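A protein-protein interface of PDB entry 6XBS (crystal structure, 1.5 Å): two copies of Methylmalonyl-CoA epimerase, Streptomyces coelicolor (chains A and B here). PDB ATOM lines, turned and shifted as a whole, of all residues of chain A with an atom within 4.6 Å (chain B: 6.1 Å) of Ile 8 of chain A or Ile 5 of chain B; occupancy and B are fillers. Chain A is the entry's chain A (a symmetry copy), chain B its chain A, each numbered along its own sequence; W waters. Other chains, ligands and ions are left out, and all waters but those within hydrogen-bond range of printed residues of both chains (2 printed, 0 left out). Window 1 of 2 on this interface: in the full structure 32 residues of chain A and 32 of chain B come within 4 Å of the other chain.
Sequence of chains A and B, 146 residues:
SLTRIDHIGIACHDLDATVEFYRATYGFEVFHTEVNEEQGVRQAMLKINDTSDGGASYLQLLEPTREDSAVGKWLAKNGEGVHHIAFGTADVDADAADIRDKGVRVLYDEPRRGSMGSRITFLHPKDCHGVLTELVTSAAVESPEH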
ATOM      1  N   HIS A   7      21.254  -8.435  13.481  1.00  0.00           N
ATOM      2  CA  HIS A   7      21.747  -7.212  14.110  1.00  0.00           C
ATOM      3  C   HIS A   7      22.879  -7.505  15.077  1.00  0.00           C
ATOM      4  O   HIS A   7      23.116  -8.676  15.466  1.00  0.00           O
ATOM      5  CB  HIS A   7      20.631  -6.444  14.837  1.00  0.00           C
ATOM      6  CG  HIS A   7      19.958  -7.114  15.977  1.00  0.00           C
ATOM      7  ND1 HIS A   7      18.794  -7.820  15.765  1.00  0.00           N
ATOM      8  CD2 HIS A   7      20.165  -7.066  17.316  1.00  0.00           C
ATOM      9  CE1 HIS A   7      18.351  -8.216  16.972  1.00  0.00           C
ATOM     10  NE2 HIS A   7      19.149  -7.797  17.935  1.00  0.00           N
ATOM     11  N   ILE A   8      23.581  -6.446  15.452  1.00  0.00           N
ATOM     12  CA  ILE A   8      24.583  -6.438  16.527  1.00  0.00           C
ATOM     13  C   ILE A   8      23.993  -5.655  17.679  1.00  0.00           C
ATOM     14  O   ILE A   8      23.614  -4.468  17.445  1.00  0.00           O
ATOM     15  CB  ILE A   8      25.902  -5.819  16.043  1.00  0.00           C
ATOM     16  CG1 ILE A   8      26.376  -6.563  14.792  1.00  0.00           C
ATOM     17  CG2 ILE A   8      26.936  -5.875  17.184  1.00  0.00           C
ATOM     18  CD1 ILE A   8      27.552  -5.940  14.042  1.00  0.00           C
ATOM     19  N   GLY A   9      23.845  -6.238  18.840  1.00  0.00           N
ATOM     20  CA  GLY A   9      23.363  -5.548  20.034  1.00  0.00           C
ATOM     21  C   GLY A   9      24.482  -4.884  20.776  1.00  0.00           C
ATOM     22  O   GLY A   9      25.424  -5.586  21.219  1.00  0.00           O
ATOM     23  N   ILE A  10      24.425  -3.568  20.870  1.00  0.00           N
ATOM     24  CA  ILE A  10      25.504  -2.752  21.466  1.00  0.00           C
ATOM     25  C   ILE A  10      24.958  -2.015  22.664  1.00  0.00           C
ATOM     26  O   ILE A  10      23.994  -1.238  22.484  1.00  0.00           O
ATOM     27  CB  ILE A  10      26.040  -1.789  20.404  1.00  0.00           C
ATOM     28  CG1 ILE A  10      26.677  -2.582  19.252  1.00  0.00           C
ATOM     29  CG2 ILE A  10      26.994  -0.790  21.015  1.00  0.00           C
ATOM     30  CD1 ILE A  10      27.045  -1.757  18.066  1.00  0.00           C
ATOM     31  N   ILE A  48      21.805  -0.826   8.339  1.00  0.00           N
ATOM     32  CA  ILE A  48      23.073  -0.693   7.620  1.00  0.00           C
ATOM     33  C   ILE A  48      22.920  -1.191   6.195  1.00  0.00           C
ATOM     34  O   ILE A  48      23.521  -0.615   5.292  1.00  0.00           O
ATOM     35  CB  ILE A  48      24.198  -1.408   8.379  1.00  0.00           C
ATOM     36  CG1 ILE A  48      24.182  -1.034   9.868  1.00  0.00           C
ATOM     37  CG2 ILE A  48      25.532  -1.092   7.744  1.00  0.00           C
ATOM     38  CD1 ILE A  48      24.168   0.415  10.153  1.00  0.00           C
ATOM     39  N   ASN A  49      22.161  -2.262   5.951  1.00  0.00           N
ATOM     40  CA  ASN A  49      22.022  -2.887   4.633  1.00  0.00           C
ATOM     41  C   ASN A  49      20.789  -3.758   4.600  1.00  0.00           C
ATOM     42  O   ASN A  49      20.328  -4.229   5.650  1.00  0.00           O
ATOM     43  CB  ASN A  49      23.291  -3.595   4.174  1.00  0.00           C
ATOM     44  CG  ASN A  49      23.757  -4.677   5.127  1.00  0.00           C
ATOM     45  OD1 ASN A  49      24.525  -4.403   6.061  1.00  0.00           O
ATOM     46  ND2 ASN A  49      23.267  -5.888   4.928  1.00  0.00           N
ATOM     47  N   SER A  57      20.020  -5.905   7.997  1.00  0.00           N
ATOM     48  CA  SER A  57      21.019  -5.947   9.093  1.00  0.00           C
ATOM     49  C   SER A  57      21.081  -4.583   9.743  1.00  0.00           C
ATOM     50  O   SER A  57      21.189  -3.571   9.030  1.00  0.00           O
ATOM     51  CB  SER A  57      22.388  -6.351   8.648  1.00  0.00           C
ATOM     52  OG  SER A  57      22.458  -7.671   8.119  1.00  0.00           O
ATOM     53  N   TYR A  58      21.034  -4.563  11.077  1.00  0.00           N
ATOM     54  CA  TYR A  58      20.973  -3.359  11.879  1.00  0.00           C
ATOM     55  C   TYR A  58      22.069  -3.338  12.926  1.00  0.00           C
ATOM     56  O   TYR A  58      22.541  -4.409  13.371  1.00  0.00           O
ATOM     57  CB  TYR A  58      19.630  -3.259  12.613  1.00  0.00           C
ATOM     58  CG  TYR A  58      18.382  -3.414  11.761  1.00  0.00           C
ATOM     59  CD1 TYR A  58      17.856  -4.639  11.448  1.00  0.00           C
ATOM     60  CD2 TYR A  58      17.719  -2.292  11.297  1.00  0.00           C
ATOM     61  CE1 TYR A  58      16.673  -4.753  10.727  1.00  0.00           C
ATOM     62  CE2 TYR A  58      16.566  -2.390  10.549  1.00  0.00           C
ATOM     63  CZ  TYR A  58      16.026  -3.614  10.305  1.00  0.00           C
ATOM     64  OH  TYR A  58      14.886  -3.796   9.541  1.00  0.00           O
ATOM     65  N   LEU A  59      22.360  -2.146  13.422  1.00  0.00           N
ATOM     66  CA  LEU A  59      22.960  -1.948  14.759  1.00  0.00           C
ATOM     67  C   LEU A  59      21.823  -1.692  15.701  1.00  0.00           C
ATOM     68  O   LEU A  59      20.943  -0.808  15.413  1.00  0.00           O
ATOM     69  CB  LEU A  59      23.960  -0.805  14.773  1.00  0.00           C
ATOM     70  CG  LEU A  59      25.061  -0.922  13.743  1.00  0.00           C
ATOM     71  CD1 LEU A  59      25.921   0.325  13.827  1.00  0.00           C
ATOM     72  CD2 LEU A  59      25.900  -2.147  13.963  1.00  0.00           C
ATOM     73  N   GLN A  60      21.734  -2.439  16.784  1.00  0.00           N
ATOM     74  CA  GLN A  60      20.714  -2.247  17.830  1.00  0.00           C
ATOM     75  C   GLN A  60      21.417  -1.658  19.045  1.00  0.00           C
ATOM     76  O   GLN A  60      22.111  -2.383  19.777  1.00  0.00           O
ATOM     77  CB  GLN A  60      20.045  -3.572  18.136  1.00  0.00           C
ATOM     78  CG  GLN A  60      18.856  -3.461  19.077  1.00  0.00           C
ATOM     79  CD  GLN A  60      18.222  -4.819  19.291  1.00  0.00           C
ATOM     80  OE1 GLN A  60      18.746  -5.643  20.075  1.00  0.00           O
ATOM     81  NE2 GLN A  60      17.122  -5.102  18.602  1.00  0.00           N
ATOM     82  N   VAL A  82      29.860  -4.320  22.695  1.00  0.00           N
ATOM     83  CA  VAL A  82      28.966  -5.343  22.108  1.00  0.00           C
ATOM     84  C   VAL A  82      28.410  -6.268  23.167  1.00  0.00           C
ATOM     85  O   VAL A  82      29.247  -6.882  23.918  1.00  0.00           O
ATOM     86  CB  VAL A  82      29.676  -6.125  21.001  1.00  0.00           C
ATOM     87  CG1 VAL A  82      28.784  -7.224  20.452  1.00  0.00           C
ATOM     88  CG2 VAL A  82      30.166  -5.257  19.853  1.00  0.00           C
ATOM     89  N   HIS A  84      25.491  -8.549  22.349  1.00  0.00           N
ATOM     90  CA  HIS A  84      25.013  -9.813  21.752  1.00  0.00           C
ATOM     91  C   HIS A  84      25.054  -9.707  20.238  1.00  0.00           C
ATOM     92  O   HIS A  84      25.179  -8.592  19.697  1.00  0.00           O
ATOM     93  CB  HIS A  84      23.601 -10.187  22.234  1.00  0.00           C
ATOM     94  CG  HIS A  84      22.527  -9.224  21.875  1.00  0.00           C
ATOM     95  ND1 HIS A  84      22.130  -8.192  22.748  1.00  0.00           N
ATOM     96  CD2 HIS A  84      21.668  -9.230  20.841  1.00  0.00           C
ATOM     97  CE1 HIS A  84      21.095  -7.600  22.138  1.00  0.00           C
ATOM     98  NE2 HIS A  84      20.772  -8.180  21.032  1.00  0.00           N
ATOM     99  N   THR B   3      28.561   0.821   3.781  1.00  0.00           N
ATOM    100  CA  THR B   3      27.363   0.334   3.097  1.00  0.00           C
ATOM    101  C   THR B   3      26.925  -1.042   3.579  1.00  0.00           C
ATOM    102  O   THR B   3      25.857  -1.512   3.110  1.00  0.00           O
ATOM    103  CB  THR B   3      27.559   0.319   1.587  1.00  0.00           C
ATOM    104  OG1 THR B   3      28.737  -0.396   1.248  1.00  0.00           O
ATOM    105  CG2 THR B   3      27.672   1.748   1.111  1.00  0.00           C
ATOM    106  N   ARG B   4      27.696  -1.718   4.467  1.00  0.00           N
ATOM    107  CA  ARG B   4      27.252  -3.002   5.013  1.00  0.00           C
ATOM    108  C   ARG B   4      27.931  -3.282   6.318  1.00  0.00           C
ATOM    109  O   ARG B   4      28.995  -2.709   6.597  1.00  0.00           O
ATOM    110  CB  ARG B   4      27.558  -4.156   4.063  1.00  0.00           C
ATOM    111  CG  ARG B   4      29.017  -4.428   3.826  1.00  0.00           C
ATOM    112  CD  ARG B   4      29.308  -5.613   2.925  1.00  0.00           C
ATOM    113  NE  ARG B   4      30.703  -5.809   2.729  1.00  0.00           N
ATOM    114  CZ  ARG B   4      31.461  -5.058   1.927  1.00  0.00           C
ATOM    115  NH1 ARG B   4      30.906  -4.158   1.161  1.00  0.00           N
ATOM    116  NH2 ARG B   4      32.769  -5.278   1.895  1.00  0.00           N
ATOM    117  N   ILE B   5      27.332  -4.191   7.076  1.00  0.00           N
ATOM    118  CA  ILE B   5      28.091  -4.933   8.108  1.00  0.00           C
ATOM    119  C   ILE B   5      28.891  -5.991   7.341  1.00  0.00           C
ATOM    120  O   ILE B   5      28.273  -6.895   6.693  1.00  0.00           O
ATOM    121  CB  ILE B   5      27.169  -5.527   9.157  1.00  0.00           C
ATOM    122  CG1 ILE B   5      26.428  -4.422   9.883  1.00  0.00           C
ATOM    123  CG2 ILE B   5      28.000  -6.466  10.050  1.00  0.00           C
ATOM    124  CD1 ILE B   5      25.373  -4.831  10.925  1.00  0.00           C
ATOM    125  N   ASP B   6      30.194  -5.931   7.334  1.00  0.00           N
ATOM    126  CA  ASP B   6      31.043  -6.917   6.640  1.00  0.00           C
ATOM    127  C   ASP B   6      31.210  -8.156   7.489  1.00  0.00           C
ATOM    128  O   ASP B   6      31.065  -9.263   6.975  1.00  0.00           O
ATOM    129  CB  ASP B   6      32.383  -6.321   6.221  1.00  0.00           C
ATOM    130  CG  ASP B   6      33.160  -7.270   5.329  1.00  0.00           C
ATOM    131  OD1 ASP B   6      32.892  -7.234   4.063  1.00  0.00           O
ATOM    132  OD2 ASP B   6      34.005  -8.034   5.810  1.00  0.00           O
ATOM    133  N   HIS B   7      31.538  -8.013   8.754  1.00  0.00           N
ATOM    134  CA  HIS B   7      31.708  -9.213   9.571  1.00  0.00           C
ATOM    135  C   HIS B   7      31.700  -8.881  11.051  1.00  0.00           C
ATOM    136  O   HIS B   7      31.825  -7.698  11.454  1.00  0.00           O
ATOM    137  CB  HIS B   7      32.996  -9.975   9.220  1.00  0.00           C
ATOM    138  CG  HIS B   7      34.291  -9.283   9.435  1.00  0.00           C
ATOM    139  ND1 HIS B   7      34.881  -8.598   8.395  1.00  0.00           N
ATOM    140  CD2 HIS B   7      35.172  -9.293  10.466  1.00  0.00           C
ATOM    141  CE1 HIS B   7      36.080  -8.176   8.835  1.00  0.00           C
ATOM    142  NE2 HIS B   7      36.295  -8.558  10.079  1.00  0.00           N
ATOM    143  N   ILE B   8      31.539  -9.921  11.857  1.00  0.00           N
ATOM    144  CA  ILE B   8      31.700  -9.888  13.316  1.00  0.00           C
ATOM    145  C   ILE B   8      32.967 -10.648  13.641  1.00  0.00           C
ATOM    146  O   ILE B   8      33.052 -11.845  13.232  1.00  0.00           O
ATOM    147  CB  ILE B   8      30.480 -10.504  14.017  1.00  0.00           C
ATOM    148  CG1 ILE B   8      29.214  -9.788  13.541  1.00  0.00           C
ATOM    149  CG2 ILE B   8      30.670 -10.405  15.543  1.00  0.00           C
ATOM    150  CD1 ILE B   8      27.887 -10.416  13.961  1.00  0.00           C
ATOM    151  N   THR B  51      24.785  -9.141   0.725  1.00  0.00           N
ATOM    152  CA  THR B  51      24.256  -7.814   1.088  1.00  0.00           C
ATOM    153  C   THR B  51      23.943  -6.932  -0.121  1.00  0.00           C
ATOM    154  O   THR B  51      24.446  -7.202  -1.248  1.00  0.00           O
ATOM    155  CB  THR B  51      25.277  -7.121   1.993  1.00  0.00           C
ATOM    156  OG1 THR B  51      26.552  -6.951   1.383  1.00  0.00           O
ATOM    157  CG2 THR B  51      25.516  -7.891   3.269  1.00  0.00           C
ATOM    158  N   ALA B  56      29.035  -9.089   1.190  1.00  0.00           N
ATOM    159  CA  ALA B  56      28.565 -10.199   2.004  1.00  0.00           C
ATOM    160  C   ALA B  56      28.836  -9.899   3.470  1.00  0.00           C
ATOM    161  O   ALA B  56      29.615  -9.005   3.781  1.00  0.00           O
ATOM    162  CB  ALA B  56      29.231 -11.484   1.616  1.00  0.00           C
ATOM    163  N   SER B  57      28.217 -10.704   4.313  1.00  0.00           N
ATOM    164  CA  SER B  57      28.396 -10.620   5.784  1.00  0.00           C
ATOM    165  C   SER B  57      28.864 -11.965   6.290  1.00  0.00           C
ATOM    166  O   SER B  57      28.266 -12.995   5.934  1.00  0.00           O
ATOM    167  CB  SER B  57      27.160 -10.212   6.520  1.00  0.00           C
ATOM    168  OG  SER B  57      26.698  -8.905   6.193  1.00  0.00           O
ATOM    169  N   TYR B  58      29.907 -11.951   7.124  1.00  0.00           N
ATOM    170  CA  TYR B  58      30.569 -13.133   7.633  1.00  0.00           C
ATOM    171  C   TYR B  58      30.648 -13.113   9.147  1.00  0.00           C
ATOM    172  O   TYR B  58      30.665 -12.025   9.766  1.00  0.00           O
ATOM    173  CB  TYR B  58      32.003 -13.230   7.096  1.00  0.00           C
ATOM    174  CG  TYR B  58      32.169 -13.114   5.591  1.00  0.00           C
ATOM    175  CD1 TYR B  58      32.259 -11.903   4.955  1.00  0.00           C
ATOM    176  CD2 TYR B  58      32.262 -14.255   4.816  1.00  0.00           C
ATOM    177  CE1 TYR B  58      32.483 -11.823   3.586  1.00  0.00           C
ATOM    178  CE2 TYR B  58      32.447 -14.192   3.451  1.00  0.00           C
ATOM    179  CZ  TYR B  58      32.600 -12.981   2.851  1.00  0.00           C
ATOM    180  OH  TYR B  58      32.761 -12.833   1.484  1.00  0.00           O
ATOM    181  N   ILE B  85      33.749  -5.440  15.405  1.00  0.00           N
ATOM    182  CA  ILE B  85      32.752  -5.408  14.319  1.00  0.00           C
ATOM    183  C   ILE B  85      33.355  -4.742  13.121  1.00  0.00           C
ATOM    184  O   ILE B  85      34.197  -3.839  13.292  1.00  0.00           O
ATOM    185  CB  ILE B  85      31.450  -4.793  14.757  1.00  0.00           C
ATOM    186  CG1 ILE B  85      31.565  -3.321  14.879  1.00  0.00           C
ATOM    187  CG2 ILE B  85      30.895  -5.389  16.024  1.00  0.00           C
ATOM    188  CD1 ILE B  85      30.186  -2.694  15.127  1.00  0.00           C
ATOM    189  N   ALA B  86      32.990  -5.104  11.904  1.00  0.00           N
ATOM    190  CA  ALA B  86      33.596  -4.550  10.677  1.00  0.00           C
ATOM    191  C   ALA B  86      32.516  -4.071   9.736  1.00  0.00           C
ATOM    192  O   ALA B  86      31.538  -4.814   9.478  1.00  0.00           O
ATOM    193  CB  ALA B  86      34.424  -5.576   9.950  1.00  0.00           C
ATOM    194  N   PHE B  87      32.704  -2.887   9.198  1.00  0.00           N
ATOM    195  CA  PHE B  87      31.819  -2.274   8.199  1.00  0.00           C
ATOM    196  C   PHE B  87      32.531  -2.274   6.854  1.00  0.00           C
ATOM    197  O   PHE B  87      33.735  -1.976   6.743  1.00  0.00           O
ATOM    198  CB  PHE B  87      31.461  -0.839   8.581  1.00  0.00           C
ATOM    199  CG  PHE B  87      30.679  -0.766   9.855  1.00  0.00           C
ATOM    200  CD1 PHE B  87      29.371  -1.146   9.936  1.00  0.00           C
ATOM    201  CD2 PHE B  87      31.260  -0.241  10.980  1.00  0.00           C
ATOM    202  CE1 PHE B  87      28.669  -1.070  11.114  1.00  0.00           C
ATOM    203  CE2 PHE B  87      30.546  -0.139  12.167  1.00  0.00           C
ATOM    204  CZ  PHE B  87      29.274  -0.618  12.243  1.00  0.00           C
ATOM    205  N   GLY B  88      31.784  -2.587   5.808  1.00  0.00           N
ATOM    206  CA  GLY B  88      32.319  -2.553   4.436  1.00  0.00           C
ATOM    207  C   GLY B  88      32.075  -1.241   3.732  1.00  0.00           C
ATOM    208  O   GLY B  88      31.080  -0.540   4.004  1.00  0.00           O
HETATM  209  O   HOH W   1      23.680  -0.050   2.196  1.00  0.00           O
HETATM  210  O   HOH W   2      24.217  -8.301   6.370  1.00  0.00           O
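Water W2 lies within hydrogen-bond range of OG of Ser 57 of chain B (2.6 Å), OG of Ser 57 of chain A (2.6 Å) and ND2 of Asn 49 of chain A (3.0 Å). Water W1 lies within hydrogen-bond range of the backbone carbonyl oxygen (O) of Thr 3 of chain B and the backbone carbonyl oxygen (O) of Ile 48 of chain A.
The backbone carbonyl oxygen (O) of Ile 5 of chain B sits at hydrogen-bond distance from the side-chain hydroxyl (OG) of Ser 57 of chain B (2.6 Å). The guanidinium group (NH2) of Arg 4 of chain B lies within salt-bridge range of the side-chain carboxylate (OD1) of Asp 6 of chain B, at 2.9 Å. The backbone carbonyl oxygen (O) of Ile 8 of chain A lies within hydrogen-bond range of the backbone NH (N) of Gln 60 of chain A. The backbone carbonyl oxygen of Arg 4 of chain B lies within hydrogen-bond range of the backbone NH of Gly 88 of chain B. The side-chain hydroxyl (OG1) of Thr 51 of chain B is in hydrogen-bond range of the backbone NH (N) of Ala 56 of chain B (3.3 Å). The backbone NH (N) of Ile 8 of chain A sits at hydrogen-bond distance from the backbone carbonyl oxygen (O) of Tyr 58 of chain A, at 3.1 Å.
His 7 of chain A touches none of the printed residues of chain B. Ile 8 of chain A touches just these residues of chain B: Ile 5 and Ile 85. Of the printed residues of chain B, Leu 59 of chain A touches Phe 87. Of the printed residues of chain A, Arg 4 of chain B touches Ile 48 (3.5 Å) and Asn 49 (3.2 Å). Of the printed residues of chain A, Ile 5 of chain B touches Ile 8 (3.96 Å), Ile 48 (3.6 Å), Asn 49 (3.0 Å) and Tyr 58 (3.8 Å). Printed residues of chain A within 4 Å of Thr 51 of chain B: Asn 49 (3.4 Å). Of the printed residues of chain A, Phe 87 of chain B touches Leu 59. The nearest residue of chain B that does not touch Ile 8 of chain A is Ile 8 of chain B (4.2 Å). The nearest printed residue of chain A that does not touch Ile 5 of chain B is Ser 57 of chain A (4.1 Å).
Positions printed for both chains: 7, 8, 57 and 58. Of the 12 pairs that touch across the chains among the printed residues, none has its exchanged pair printed and touching as well.
Ile 5 of chain B touches Ile 8 of chain A. CG2 of Ile 85 of chain B touches CD1 of Ile 8 of chain A (3.9 Å). CG2 of Ile 48 of chain A touches C of Arg 4 of chain B, 3.5 Å away. Ile 5 of chain B touches Ile 48 of chain A. O of Thr 3 of chain B touches CB of Asn 49 of chain A (3.5 Å). OD1 of Asn 49 of chain A touches CA of Arg 4 of chain B, at 3.2 Å. ND2 of Asn 49 of chain A touches CG2 of Thr 51 of chain B, 3.4 Å away. O of Tyr 58 of chain A touches CD1 of Ile 5 of chain B, 3.8 Å away. CD1 of Leu 59 of chain A touches CZ of Phe 87 of chain B, 3.8 Å away. CG2 of Ile 85 of chain B touches CG2 of Val 82 of chain A (3.9 Å).
Hydrophobic or aromatic side chains of chain B that line the printed part of chain A: Ile 5, Ile 85 and Phe 87. Printed residues of chain A that touch a printed residue of chain B: Ile 8, Ile 48, Asn 49, Tyr 58, Leu 59 and Val 82. Hydrophobic or aromatic side chains of chain A within 4 Å of the printed part of chain B: Ile 8, Ile 48, Leu 59 and Val 82. Among the printed residues, no Asp or Glu carboxylate lies within 4 Å of a Lys or Arg side-chain nitrogen of the other chain.
O of Thr 3 of chain B sits close to O of Ile 48 of chain A, 3.3 Å away. The backbone NH of Ile 5 of chain B lies within hydrogen-bond range of the side-chain amide oxygen of Asn 49 of chain A (3.0 Å).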
